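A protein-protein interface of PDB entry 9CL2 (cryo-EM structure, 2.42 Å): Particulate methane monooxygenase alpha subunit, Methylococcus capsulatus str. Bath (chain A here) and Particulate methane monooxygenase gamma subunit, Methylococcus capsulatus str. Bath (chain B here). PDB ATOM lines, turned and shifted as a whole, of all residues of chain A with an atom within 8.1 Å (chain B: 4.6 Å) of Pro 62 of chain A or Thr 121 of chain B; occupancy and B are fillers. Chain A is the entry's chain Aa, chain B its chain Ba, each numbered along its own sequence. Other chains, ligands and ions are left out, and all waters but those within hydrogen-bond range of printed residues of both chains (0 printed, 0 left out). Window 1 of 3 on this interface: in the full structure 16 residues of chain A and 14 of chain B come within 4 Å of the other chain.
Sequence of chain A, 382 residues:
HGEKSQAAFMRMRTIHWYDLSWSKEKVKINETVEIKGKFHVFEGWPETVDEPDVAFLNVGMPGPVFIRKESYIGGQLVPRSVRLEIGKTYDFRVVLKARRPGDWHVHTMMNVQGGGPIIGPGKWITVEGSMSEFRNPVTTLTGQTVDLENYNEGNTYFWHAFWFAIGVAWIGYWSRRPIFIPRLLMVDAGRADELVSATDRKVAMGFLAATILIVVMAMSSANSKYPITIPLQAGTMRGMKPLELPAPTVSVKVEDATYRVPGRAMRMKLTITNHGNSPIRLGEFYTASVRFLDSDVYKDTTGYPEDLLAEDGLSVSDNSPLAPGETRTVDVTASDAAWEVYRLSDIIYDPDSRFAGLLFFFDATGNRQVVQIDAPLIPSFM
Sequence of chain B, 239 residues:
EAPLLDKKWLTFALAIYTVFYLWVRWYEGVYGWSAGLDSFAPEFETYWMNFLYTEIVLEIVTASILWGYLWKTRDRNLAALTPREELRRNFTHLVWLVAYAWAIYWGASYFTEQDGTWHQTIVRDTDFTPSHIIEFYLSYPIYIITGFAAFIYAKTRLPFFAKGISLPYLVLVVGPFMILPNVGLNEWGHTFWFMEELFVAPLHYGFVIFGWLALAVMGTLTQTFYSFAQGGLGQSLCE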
ATOM      1  N   HIS A   1      -9.130  -0.911  -1.321  1.00  0.00           N
ATOM      2  CA  HIS A   1      -8.770   0.508  -1.587  1.00  0.00           C
ATOM      3  C   HIS A   1      -9.339   1.004  -2.925  1.00  0.00           C
ATOM      4  O   HIS A   1      -9.232   0.259  -3.917  1.00  0.00           O
ATOM      5  CB  HIS A   1      -7.253   0.608  -1.471  1.00  0.00           C
ATOM      6  CG  HIS A   1      -6.796   0.098  -0.154  1.00  0.00           C
ATOM      7  ND1 HIS A   1      -7.448  -0.868   0.591  1.00  0.00           N
ATOM      8  CD2 HIS A   1      -5.731   0.478   0.552  1.00  0.00           C
ATOM      9  CE1 HIS A   1      -6.753  -1.049   1.707  1.00  0.00           C
ATOM     10  NE2 HIS A   1      -5.715  -0.249   1.703  1.00  0.00           N
ATOM     11  N   VAL A  59     -11.094 -10.084  -7.686  1.00  0.00           N
ATOM     12  CA  VAL A  59     -10.558  -9.936  -6.339  1.00  0.00           C
ATOM     13  C   VAL A  59      -9.716  -8.670  -6.302  1.00  0.00           C
ATOM     14  O   VAL A  59      -8.773  -8.520  -7.088  1.00  0.00           O
ATOM     15  CB  VAL A  59      -9.729 -11.164  -5.926  1.00  0.00           C
ATOM     16  CG1 VAL A  59      -9.306 -11.052  -4.472  1.00  0.00           C
ATOM     17  CG2 VAL A  59     -10.520 -12.439  -6.164  1.00  0.00           C
ATOM     18  N   GLY A  60     -10.059  -7.762  -5.395  1.00  0.00           N
ATOM     19  CA  GLY A  60      -9.335  -6.516  -5.252  1.00  0.00           C
ATOM     20  C   GLY A  60      -8.220  -6.611  -4.233  1.00  0.00           C
ATOM     21  O   GLY A  60      -8.473  -6.791  -3.039  1.00  0.00           O
ATOM     22  N   MET A  61      -6.984  -6.501  -4.703  1.00  0.00           N
ATOM     23  CA  MET A  61      -5.802  -6.597  -3.862  1.00  0.00           C
ATOM     24  C   MET A  61      -4.652  -5.926  -4.596  1.00  0.00           C
ATOM     25  O   MET A  61      -4.712  -5.752  -5.819  1.00  0.00           O
ATOM     26  CB  MET A  61      -5.482  -8.062  -3.525  1.00  0.00           C
ATOM     27  CG  MET A  61      -5.393  -8.988  -4.719  1.00  0.00           C
ATOM     28  SD  MET A  61      -5.578 -10.710  -4.219  1.00  0.00           S
ATOM     29  CE  MET A  61      -5.026 -11.552  -5.696  1.00  0.00           C
ATOM     30  N   PRO A  62      -3.583  -5.532  -3.881  1.00  0.00           N
ATOM     31  CA  PRO A  62      -2.550  -4.698  -4.517  1.00  0.00           C
ATOM     32  C   PRO A  62      -1.700  -5.439  -5.540  1.00  0.00           C
ATOM     33  O   PRO A  62      -0.688  -4.909  -6.010  1.00  0.00           O
ATOM     34  CB  PRO A  62      -1.694  -4.218  -3.336  1.00  0.00           C
ATOM     35  CG  PRO A  62      -2.024  -5.089  -2.198  1.00  0.00           C
ATOM     36  CD  PRO A  62      -3.344  -5.731  -2.439  1.00  0.00           C
ATOM     37  N   GLY A  63      -2.095  -6.656  -5.893  1.00  0.00           N
ATOM     38  CA  GLY A  63      -1.388  -7.431  -6.881  1.00  0.00           C
ATOM     39  C   GLY A  63      -1.582  -8.914  -6.658  1.00  0.00           C
ATOM     40  O   GLY A  63      -2.480  -9.339  -5.925  1.00  0.00           O
ATOM     41  N   PRO A  64      -0.742  -9.735  -7.280  1.00  0.00           N
ATOM     42  CA  PRO A  64      -0.805 -11.189  -7.081  1.00  0.00           C
ATOM     43  C   PRO A  64      -0.195 -11.643  -5.755  1.00  0.00           C
ATOM     44  O   PRO A  64       0.600 -12.583  -5.705  1.00  0.00           O
ATOM     45  CB  PRO A  64      -0.034 -11.737  -8.285  1.00  0.00           C
ATOM     46  CG  PRO A  64       0.744 -10.600  -8.853  1.00  0.00           C
ATOM     47  CD  PRO A  64       0.345  -9.329  -8.185  1.00  0.00           C
ATOM     48  N   VAL A  65      -0.570 -10.963  -4.669  1.00  0.00           N
ATOM     49  CA  VAL A  65      -0.200 -11.431  -3.338  1.00  0.00           C
ATOM     50  C   VAL A  65      -0.918 -12.736  -3.030  1.00  0.00           C
ATOM     51  O   VAL A  65      -0.412 -13.574  -2.276  1.00  0.00           O
ATOM     52  CB  VAL A  65      -0.497 -10.347  -2.286  1.00  0.00           C
ATOM     53  CG1 VAL A  65       0.388  -9.136  -2.521  1.00  0.00           C
ATOM     54  CG2 VAL A  65      -1.964  -9.949  -2.325  1.00  0.00           C
ATOM     55  N   PHE A  66      -2.106 -12.918  -3.594  1.00  0.00           N
ATOM     56  CA  PHE A  66      -2.777 -14.201  -3.689  1.00  0.00           C
ATOM     57  C   PHE A  66      -2.889 -14.584  -5.158  1.00  0.00           C
ATOM     58  O   PHE A  66      -2.712 -13.754  -6.053  1.00  0.00           O
ATOM     59  CB  PHE A  66      -4.177 -14.152  -3.063  1.00  0.00           C
ATOM     60  CG  PHE A  66      -4.177 -14.009  -1.570  1.00  0.00           C
ATOM     61  CD1 PHE A  66      -4.133 -12.757  -0.980  1.00  0.00           C
ATOM     62  CD2 PHE A  66      -4.237 -15.125  -0.756  1.00  0.00           C
ATOM     63  CE1 PHE A  66      -4.139 -12.624   0.393  1.00  0.00           C
ATOM     64  CE2 PHE A  66      -4.243 -14.999   0.618  1.00  0.00           C
ATOM     65  CZ  PHE A  66      -4.195 -13.747   1.193  1.00  0.00           C
ATOM     66  N   ARG A 100       2.317 -14.182  -1.320  1.00  0.00           N
ATOM     67  CA  ARG A 100       3.302 -13.269  -0.765  1.00  0.00           C
ATOM     68  C   ARG A 100       2.976 -12.932   0.684  1.00  0.00           C
ATOM     69  O   ARG A 100       1.805 -12.735   1.028  1.00  0.00           O
ATOM     70  CB  ARG A 100       3.373 -11.972  -1.586  1.00  0.00           C
ATOM     71  CG  ARG A 100       3.865 -12.169  -3.009  1.00  0.00           C
ATOM     72  CD  ARG A 100       4.185 -10.842  -3.676  1.00  0.00           C
ATOM     73  NE  ARG A 100       4.757  -9.882  -2.740  1.00  0.00           N
ATOM     74  CZ  ARG A 100       4.519  -8.578  -2.767  1.00  0.00           C
ATOM     75  NH1 ARG A 100       3.717  -8.040  -3.670  1.00  0.00           N
ATOM     76  NH2 ARG A 100       5.101  -7.794  -1.864  1.00  0.00           N
ATOM     77  N   ASP A 103       0.411  -8.127   5.350  1.00  0.00           N
ATOM     78  CA  ASP A 103      -1.021  -7.893   5.678  1.00  0.00           C
ATOM     79  C   ASP A 103      -1.705  -7.324   4.439  1.00  0.00           C
ATOM     80  O   ASP A 103      -1.248  -6.282   3.947  1.00  0.00           O
ATOM     81  CB  ASP A 103      -1.177  -7.057   6.934  1.00  0.00           C
ATOM     82  CG  ASP A 103      -2.219  -7.577   7.912  1.00  0.00           C
ATOM     83  OD1 ASP A 103      -3.388  -7.719   7.501  1.00  0.00           O
ATOM     84  OD2 ASP A 103      -1.846  -7.854   9.069  1.00  0.00           O
ATOM     85  N   TRP A 104      -2.746  -7.995   3.959  1.00  0.00           N
ATOM     86  CA  TRP A 104      -3.372  -7.564   2.688  1.00  0.00           C
ATOM     87  C   TRP A 104      -4.854  -7.290   2.880  1.00  0.00           C
ATOM     88  O   TRP A 104      -5.531  -8.112   3.510  1.00  0.00           O
ATOM     89  CB  TRP A 104      -3.137  -8.638   1.620  1.00  0.00           C
ATOM     90  CG  TRP A 104      -1.703  -9.077   1.504  1.00  0.00           C
ATOM     91  CD1 TRP A 104      -1.184 -10.297   1.820  1.00  0.00           C
ATOM     92  CD2 TRP A 104      -0.598  -8.278   1.035  1.00  0.00           C
ATOM     93  NE1 TRP A 104       0.163 -10.316   1.579  1.00  0.00           N
ATOM     94  CE2 TRP A 104       0.552  -9.093   1.100  1.00  0.00           C
ATOM     95  CE3 TRP A 104      -0.469  -6.967   0.569  1.00  0.00           C
ATOM     96  CZ2 TRP A 104       1.806  -8.633   0.714  1.00  0.00           C
ATOM     97  CZ3 TRP A 104       0.774  -6.514   0.190  1.00  0.00           C
ATOM     98  CH2 TRP A 104       1.894  -7.337   0.263  1.00  0.00           C
ATOM     99  N   HIS A 105      -5.324  -6.155   2.371  1.00  0.00           N
ATOM    100  CA  HIS A 105      -6.765  -5.815   2.423  1.00  0.00           C
ATOM    101  C   HIS A 105      -7.407  -6.441   1.190  1.00  0.00           C
ATOM    102  O   HIS A 105      -7.135  -5.975   0.069  1.00  0.00           O
ATOM    103  CB  HIS A 105      -6.913  -4.298   2.457  1.00  0.00           C
ATOM    104  CG  HIS A 105      -8.181  -3.823   3.058  1.00  0.00           C
ATOM    105  ND1 HIS A 105      -8.824  -2.696   2.602  1.00  0.00           N
ATOM    106  CD2 HIS A 105      -8.916  -4.300   4.062  1.00  0.00           C
ATOM    107  CE1 HIS A 105      -9.921  -2.512   3.320  1.00  0.00           C
ATOM    108  NE2 HIS A 105      -9.992  -3.472   4.213  1.00  0.00           N
ATOM    109  N   VAL A 106      -8.209  -7.485   1.383  1.00  0.00           N
ATOM    110  CA  VAL A 106      -8.767  -8.224   0.214  1.00  0.00           C
ATOM    111  C   VAL A 106     -10.258  -7.909   0.076  1.00  0.00           C
ATOM    112  O   VAL A 106     -10.976  -8.042   1.070  1.00  0.00           O
ATOM    113  CB  VAL A 106      -8.503  -9.737   0.346  1.00  0.00           C
ATOM    114  CG1 VAL A 106      -8.997 -10.512  -0.866  1.00  0.00           C
ATOM    115  CG2 VAL A 106      -7.031 -10.031   0.606  1.00  0.00           C
ATOM    116  N   HIS A 107     -10.685  -7.536  -1.126  1.00  0.00           N
ATOM    117  CA  HIS A 107     -12.103  -7.200  -1.383  1.00  0.00           C
ATOM    118  C   HIS A 107     -12.664  -8.086  -2.485  1.00  0.00           C
ATOM    119  O   HIS A 107     -11.899  -8.552  -3.344  1.00  0.00           O
ATOM    120  CB  HIS A 107     -12.242  -5.816  -2.009  1.00  0.00           C
ATOM    121  CG  HIS A 107     -11.704  -4.678  -1.224  1.00  0.00           C
ATOM    122  ND1 HIS A 107     -12.517  -3.837  -0.499  1.00  0.00           N
ATOM    123  CD2 HIS A 107     -10.464  -4.209  -1.084  1.00  0.00           C
ATOM    124  CE1 HIS A 107     -11.775  -2.906   0.074  1.00  0.00           C
ATOM    125  NE2 HIS A 107     -10.528  -3.115  -0.272  1.00  0.00           N
ATOM    126  N   TRP A 124      -8.845  -7.587   6.193  1.00  0.00           N
ATOM    127  CA  TRP A 124      -7.399  -7.679   6.358  1.00  0.00           C
ATOM    128  C   TRP A 124      -7.014  -9.130   6.621  1.00  0.00           C
ATOM    129  O   TRP A 124      -7.516  -9.750   7.565  1.00  0.00           O
ATOM    130  CB  TRP A 124      -6.926  -6.780   7.499  1.00  0.00           C
ATOM    131  CG  TRP A 124      -6.947  -5.320   7.164  1.00  0.00           C
ATOM    132  CD1 TRP A 124      -7.901  -4.412   7.519  1.00  0.00           C
ATOM    133  CD2 TRP A 124      -5.967  -4.599   6.407  1.00  0.00           C
ATOM    134  NE1 TRP A 124      -7.577  -3.171   7.028  1.00  0.00           N
ATOM    135  CE2 TRP A 124      -6.394  -3.259   6.343  1.00  0.00           C
ATOM    136  CE3 TRP A 124      -4.771  -4.957   5.780  1.00  0.00           C
ATOM    137  CZ2 TRP A 124      -5.668  -2.276   5.676  1.00  0.00           C
ATOM    138  CZ3 TRP A 124      -4.052  -3.980   5.116  1.00  0.00           C
ATOM    139  CH2 TRP A 124      -4.503  -2.656   5.070  1.00  0.00           C
ATOM    140  N   TRP B  33       3.573   0.957  -1.347  1.00  0.00           N
ATOM    141  CA  TRP B  33       2.690  -0.076  -0.823  1.00  0.00           C
ATOM    142  C   TRP B  33       2.052   0.326   0.501  1.00  0.00           C
ATOM    143  O   TRP B  33       0.838   0.184   0.672  1.00  0.00           O
ATOM    144  CB  TRP B  33       3.467  -1.383  -0.647  1.00  0.00           C
ATOM    145  CG  TRP B  33       4.018  -1.920  -1.927  1.00  0.00           C
ATOM    146  CD1 TRP B  33       5.303  -1.817  -2.372  1.00  0.00           C
ATOM    147  CD2 TRP B  33       3.302  -2.639  -2.936  1.00  0.00           C
ATOM    148  NE1 TRP B  33       5.432  -2.430  -3.595  1.00  0.00           N
ATOM    149  CE2 TRP B  33       4.216  -2.941  -3.963  1.00  0.00           C
ATOM    150  CE3 TRP B  33       1.975  -3.056  -3.071  1.00  0.00           C
ATOM    151  CZ2 TRP B  33       3.847  -3.642  -5.108  1.00  0.00           C
ATOM    152  CZ3 TRP B  33       1.612  -3.752  -4.209  1.00  0.00           C
ATOM    153  CH2 TRP B  33       2.544  -4.038  -5.211  1.00  0.00           C
ATOM    154  N   LEU B  37      -1.529   3.176  -1.497  1.00  0.00           N
ATOM    155  CA  LEU B  37      -2.725   2.459  -1.930  1.00  0.00           C
ATOM    156  C   LEU B  37      -3.995   3.255  -1.648  1.00  0.00           C
ATOM    157  O   LEU B  37      -4.877   3.349  -2.511  1.00  0.00           O
ATOM    158  CB  LEU B  37      -2.790   1.089  -1.257  1.00  0.00           C
ATOM    159  CG  LEU B  37      -1.875   0.018  -1.852  1.00  0.00           C
ATOM    160  CD1 LEU B  37      -1.679  -1.131  -0.877  1.00  0.00           C
ATOM    161  CD2 LEU B  37      -2.430  -0.483  -3.176  1.00  0.00           C
ATOM    162  N   THR B 117       1.710  -0.338 -15.540  1.00  0.00           N
ATOM    163  CA  THR B 117       1.720  -1.443 -14.587  1.00  0.00           C
ATOM    164  C   THR B 117       0.878  -1.113 -13.360  1.00  0.00           C
ATOM    165  O   THR B 117      -0.031  -1.866 -12.988  1.00  0.00           O
ATOM    166  CB  THR B 117       3.157  -1.758 -14.167  1.00  0.00           C
ATOM    167  OG1 THR B 117       4.014  -1.721 -15.314  1.00  0.00           O
ATOM    168  CG2 THR B 117       3.236  -3.131 -13.522  1.00  0.00           C
ATOM    169  N   TRP B 118       1.155   0.039 -12.743  1.00  0.00           N
ATOM    170  CA  TRP B 118       0.437   0.436 -11.538  1.00  0.00           C
ATOM    171  C   TRP B 118      -1.066   0.455 -11.774  1.00  0.00           C
ATOM    172  O   TRP B 118      -1.837  -0.033 -10.943  1.00  0.00           O
ATOM    173  CB  TRP B 118       0.924   1.806 -11.065  1.00  0.00           C
ATOM    174  CG  TRP B 118       0.376   2.219  -9.734  1.00  0.00           C
ATOM    175  CD1 TRP B 118      -0.566   3.177  -9.499  1.00  0.00           C
ATOM    176  CD2 TRP B 118       0.737   1.691  -8.452  1.00  0.00           C
ATOM    177  NE1 TRP B 118      -0.815   3.278  -8.153  1.00  0.00           N
ATOM    178  CE2 TRP B 118      -0.027   2.376  -7.488  1.00  0.00           C
ATOM    179  CE3 TRP B 118       1.633   0.704  -8.028  1.00  0.00           C
ATOM    180  CZ2 TRP B 118       0.076   2.107  -6.124  1.00  0.00           C
ATOM    181  CZ3 TRP B 118       1.733   0.438  -6.674  1.00  0.00           C
ATOM    182  CH2 TRP B 118       0.960   1.137  -5.739  1.00  0.00           C
ATOM    183  N   HIS B 119      -1.502   0.986 -12.918  1.00  0.00           N
ATOM    184  CA  HIS B 119      -2.935   1.048 -13.180  1.00  0.00           C
ATOM    185  C   HIS B 119      -3.525  -0.326 -13.466  1.00  0.00           C
ATOM    186  O   HIS B 119      -4.712  -0.550 -13.202  1.00  0.00           O
ATOM    187  CB  HIS B 119      -3.221   2.002 -14.336  1.00  0.00           C
ATOM    188  CG  HIS B 119      -2.881   3.425 -14.030  1.00  0.00           C
ATOM    189  ND1 HIS B 119      -3.214   4.028 -12.836  1.00  0.00           N
ATOM    190  CD2 HIS B 119      -2.237   4.365 -14.760  1.00  0.00           C
ATOM    191  CE1 HIS B 119      -2.787   5.278 -12.843  1.00  0.00           C
ATOM    192  NE2 HIS B 119      -2.190   5.507 -13.999  1.00  0.00           N
ATOM    193  N   GLN B 120      -2.731  -1.256 -13.999  1.00  0.00           N
ATOM    194  CA  GLN B 120      -3.261  -2.599 -14.207  1.00  0.00           C
ATOM    195  C   GLN B 120      -3.258  -3.461 -12.949  1.00  0.00           C
ATOM    196  O   GLN B 120      -3.921  -4.503 -12.943  1.00  0.00           O
ATOM    197  CB  GLN B 120      -2.505  -3.333 -15.320  1.00  0.00           C
ATOM    198  CG  GLN B 120      -2.318  -2.541 -16.601  1.00  0.00           C
ATOM    199  CD  GLN B 120      -3.451  -2.745 -17.585  1.00  0.00           C
ATOM    200  OE1 GLN B 120      -4.564  -2.263 -17.377  1.00  0.00           O
ATOM    201  NE2 GLN B 120      -3.173  -3.463 -18.667  1.00  0.00           N
ATOM    202  N   THR B 121      -2.543  -3.077 -11.888  1.00  0.00           N
ATOM    203  CA  THR B 121      -2.570  -3.907 -10.684  1.00  0.00           C
ATOM    204  C   THR B 121      -3.480  -3.401  -9.568  1.00  0.00           C
ATOM    205  O   THR B 121      -3.789  -4.179  -8.659  1.00  0.00           O
ATOM    206  CB  THR B 121      -1.160  -4.104 -10.108  1.00  0.00           C
ATOM    207  OG1 THR B 121      -0.845  -3.037  -9.202  1.00  0.00           O
ATOM    208  CG2 THR B 121      -0.125  -4.211 -11.203  1.00  0.00           C
ATOM    209  N   ILE B 122      -3.921  -2.143  -9.589  1.00  0.00           N
ATOM    210  CA  ILE B 122      -4.772  -1.618  -8.527  1.00  0.00           C
ATOM    211  C   ILE B 122      -5.967  -0.897  -9.144  1.00  0.00           C
ATOM    212  O   ILE B 122      -6.046  -0.695 -10.355  1.00  0.00           O
ATOM    213  CB  ILE B 122      -4.007  -0.688  -7.559  1.00  0.00           C
ATOM    214  CG1 ILE B 122      -3.286   0.434  -8.310  1.00  0.00           C
ATOM    215  CG2 ILE B 122      -3.019  -1.486  -6.720  1.00  0.00           C
ATOM    216  CD1 ILE B 122      -4.066   1.732  -8.405  1.00  0.00           C
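O of Met 61 of chain A lies close to O of Thr 121 of chain B (3.4 Å).
Leu 37 of chain B touches His 1 of chain A.
O of Pro 62 of chain A touches CZ3 of Trp 33 of chain B, at 3.1 Å.
Leu 37 of chain B touches Pro 62 of chain A.
Pro 62 of chain A touches Thr 121 of chain B (O to OG1, 3.7 Å).
CG2 of Ile 122 of chain B touches CA of Pro 62 of chain A (3.9 Å).
Of the printed residues of chain B, His 1 of chain A touches Leu 37.
Of the printed residues of chain B, Met 61 of chain A touches Thr 121 (3.4 Å).
Pro 62 of chain A touches just these residues of chain B: Trp 33 (3.1 Å), Leu 37 (3.8 Å), Thr 121 (3.7 Å) and Ile 122 (3.9 Å).
Printed residues of chain A within 4 Å of Trp 33 of chain B: Pro 62.
Thr 121 of chain B touches just these residues of chain A: Met 61 (3.4 Å) and Pro 62 (3.7 Å).
The nearest printed residue of chain B that does not touch Pro 62 of chain A is Trp 118 of chain B (5.9 Å).
The nearest printed residue of chain B that does not touch His 1 of chain A is Ile 122 of chain B (6.3 Å).
Printed residues of chain A that touch a printed residue of chain B: His 1, Met 61 and Pro 62.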
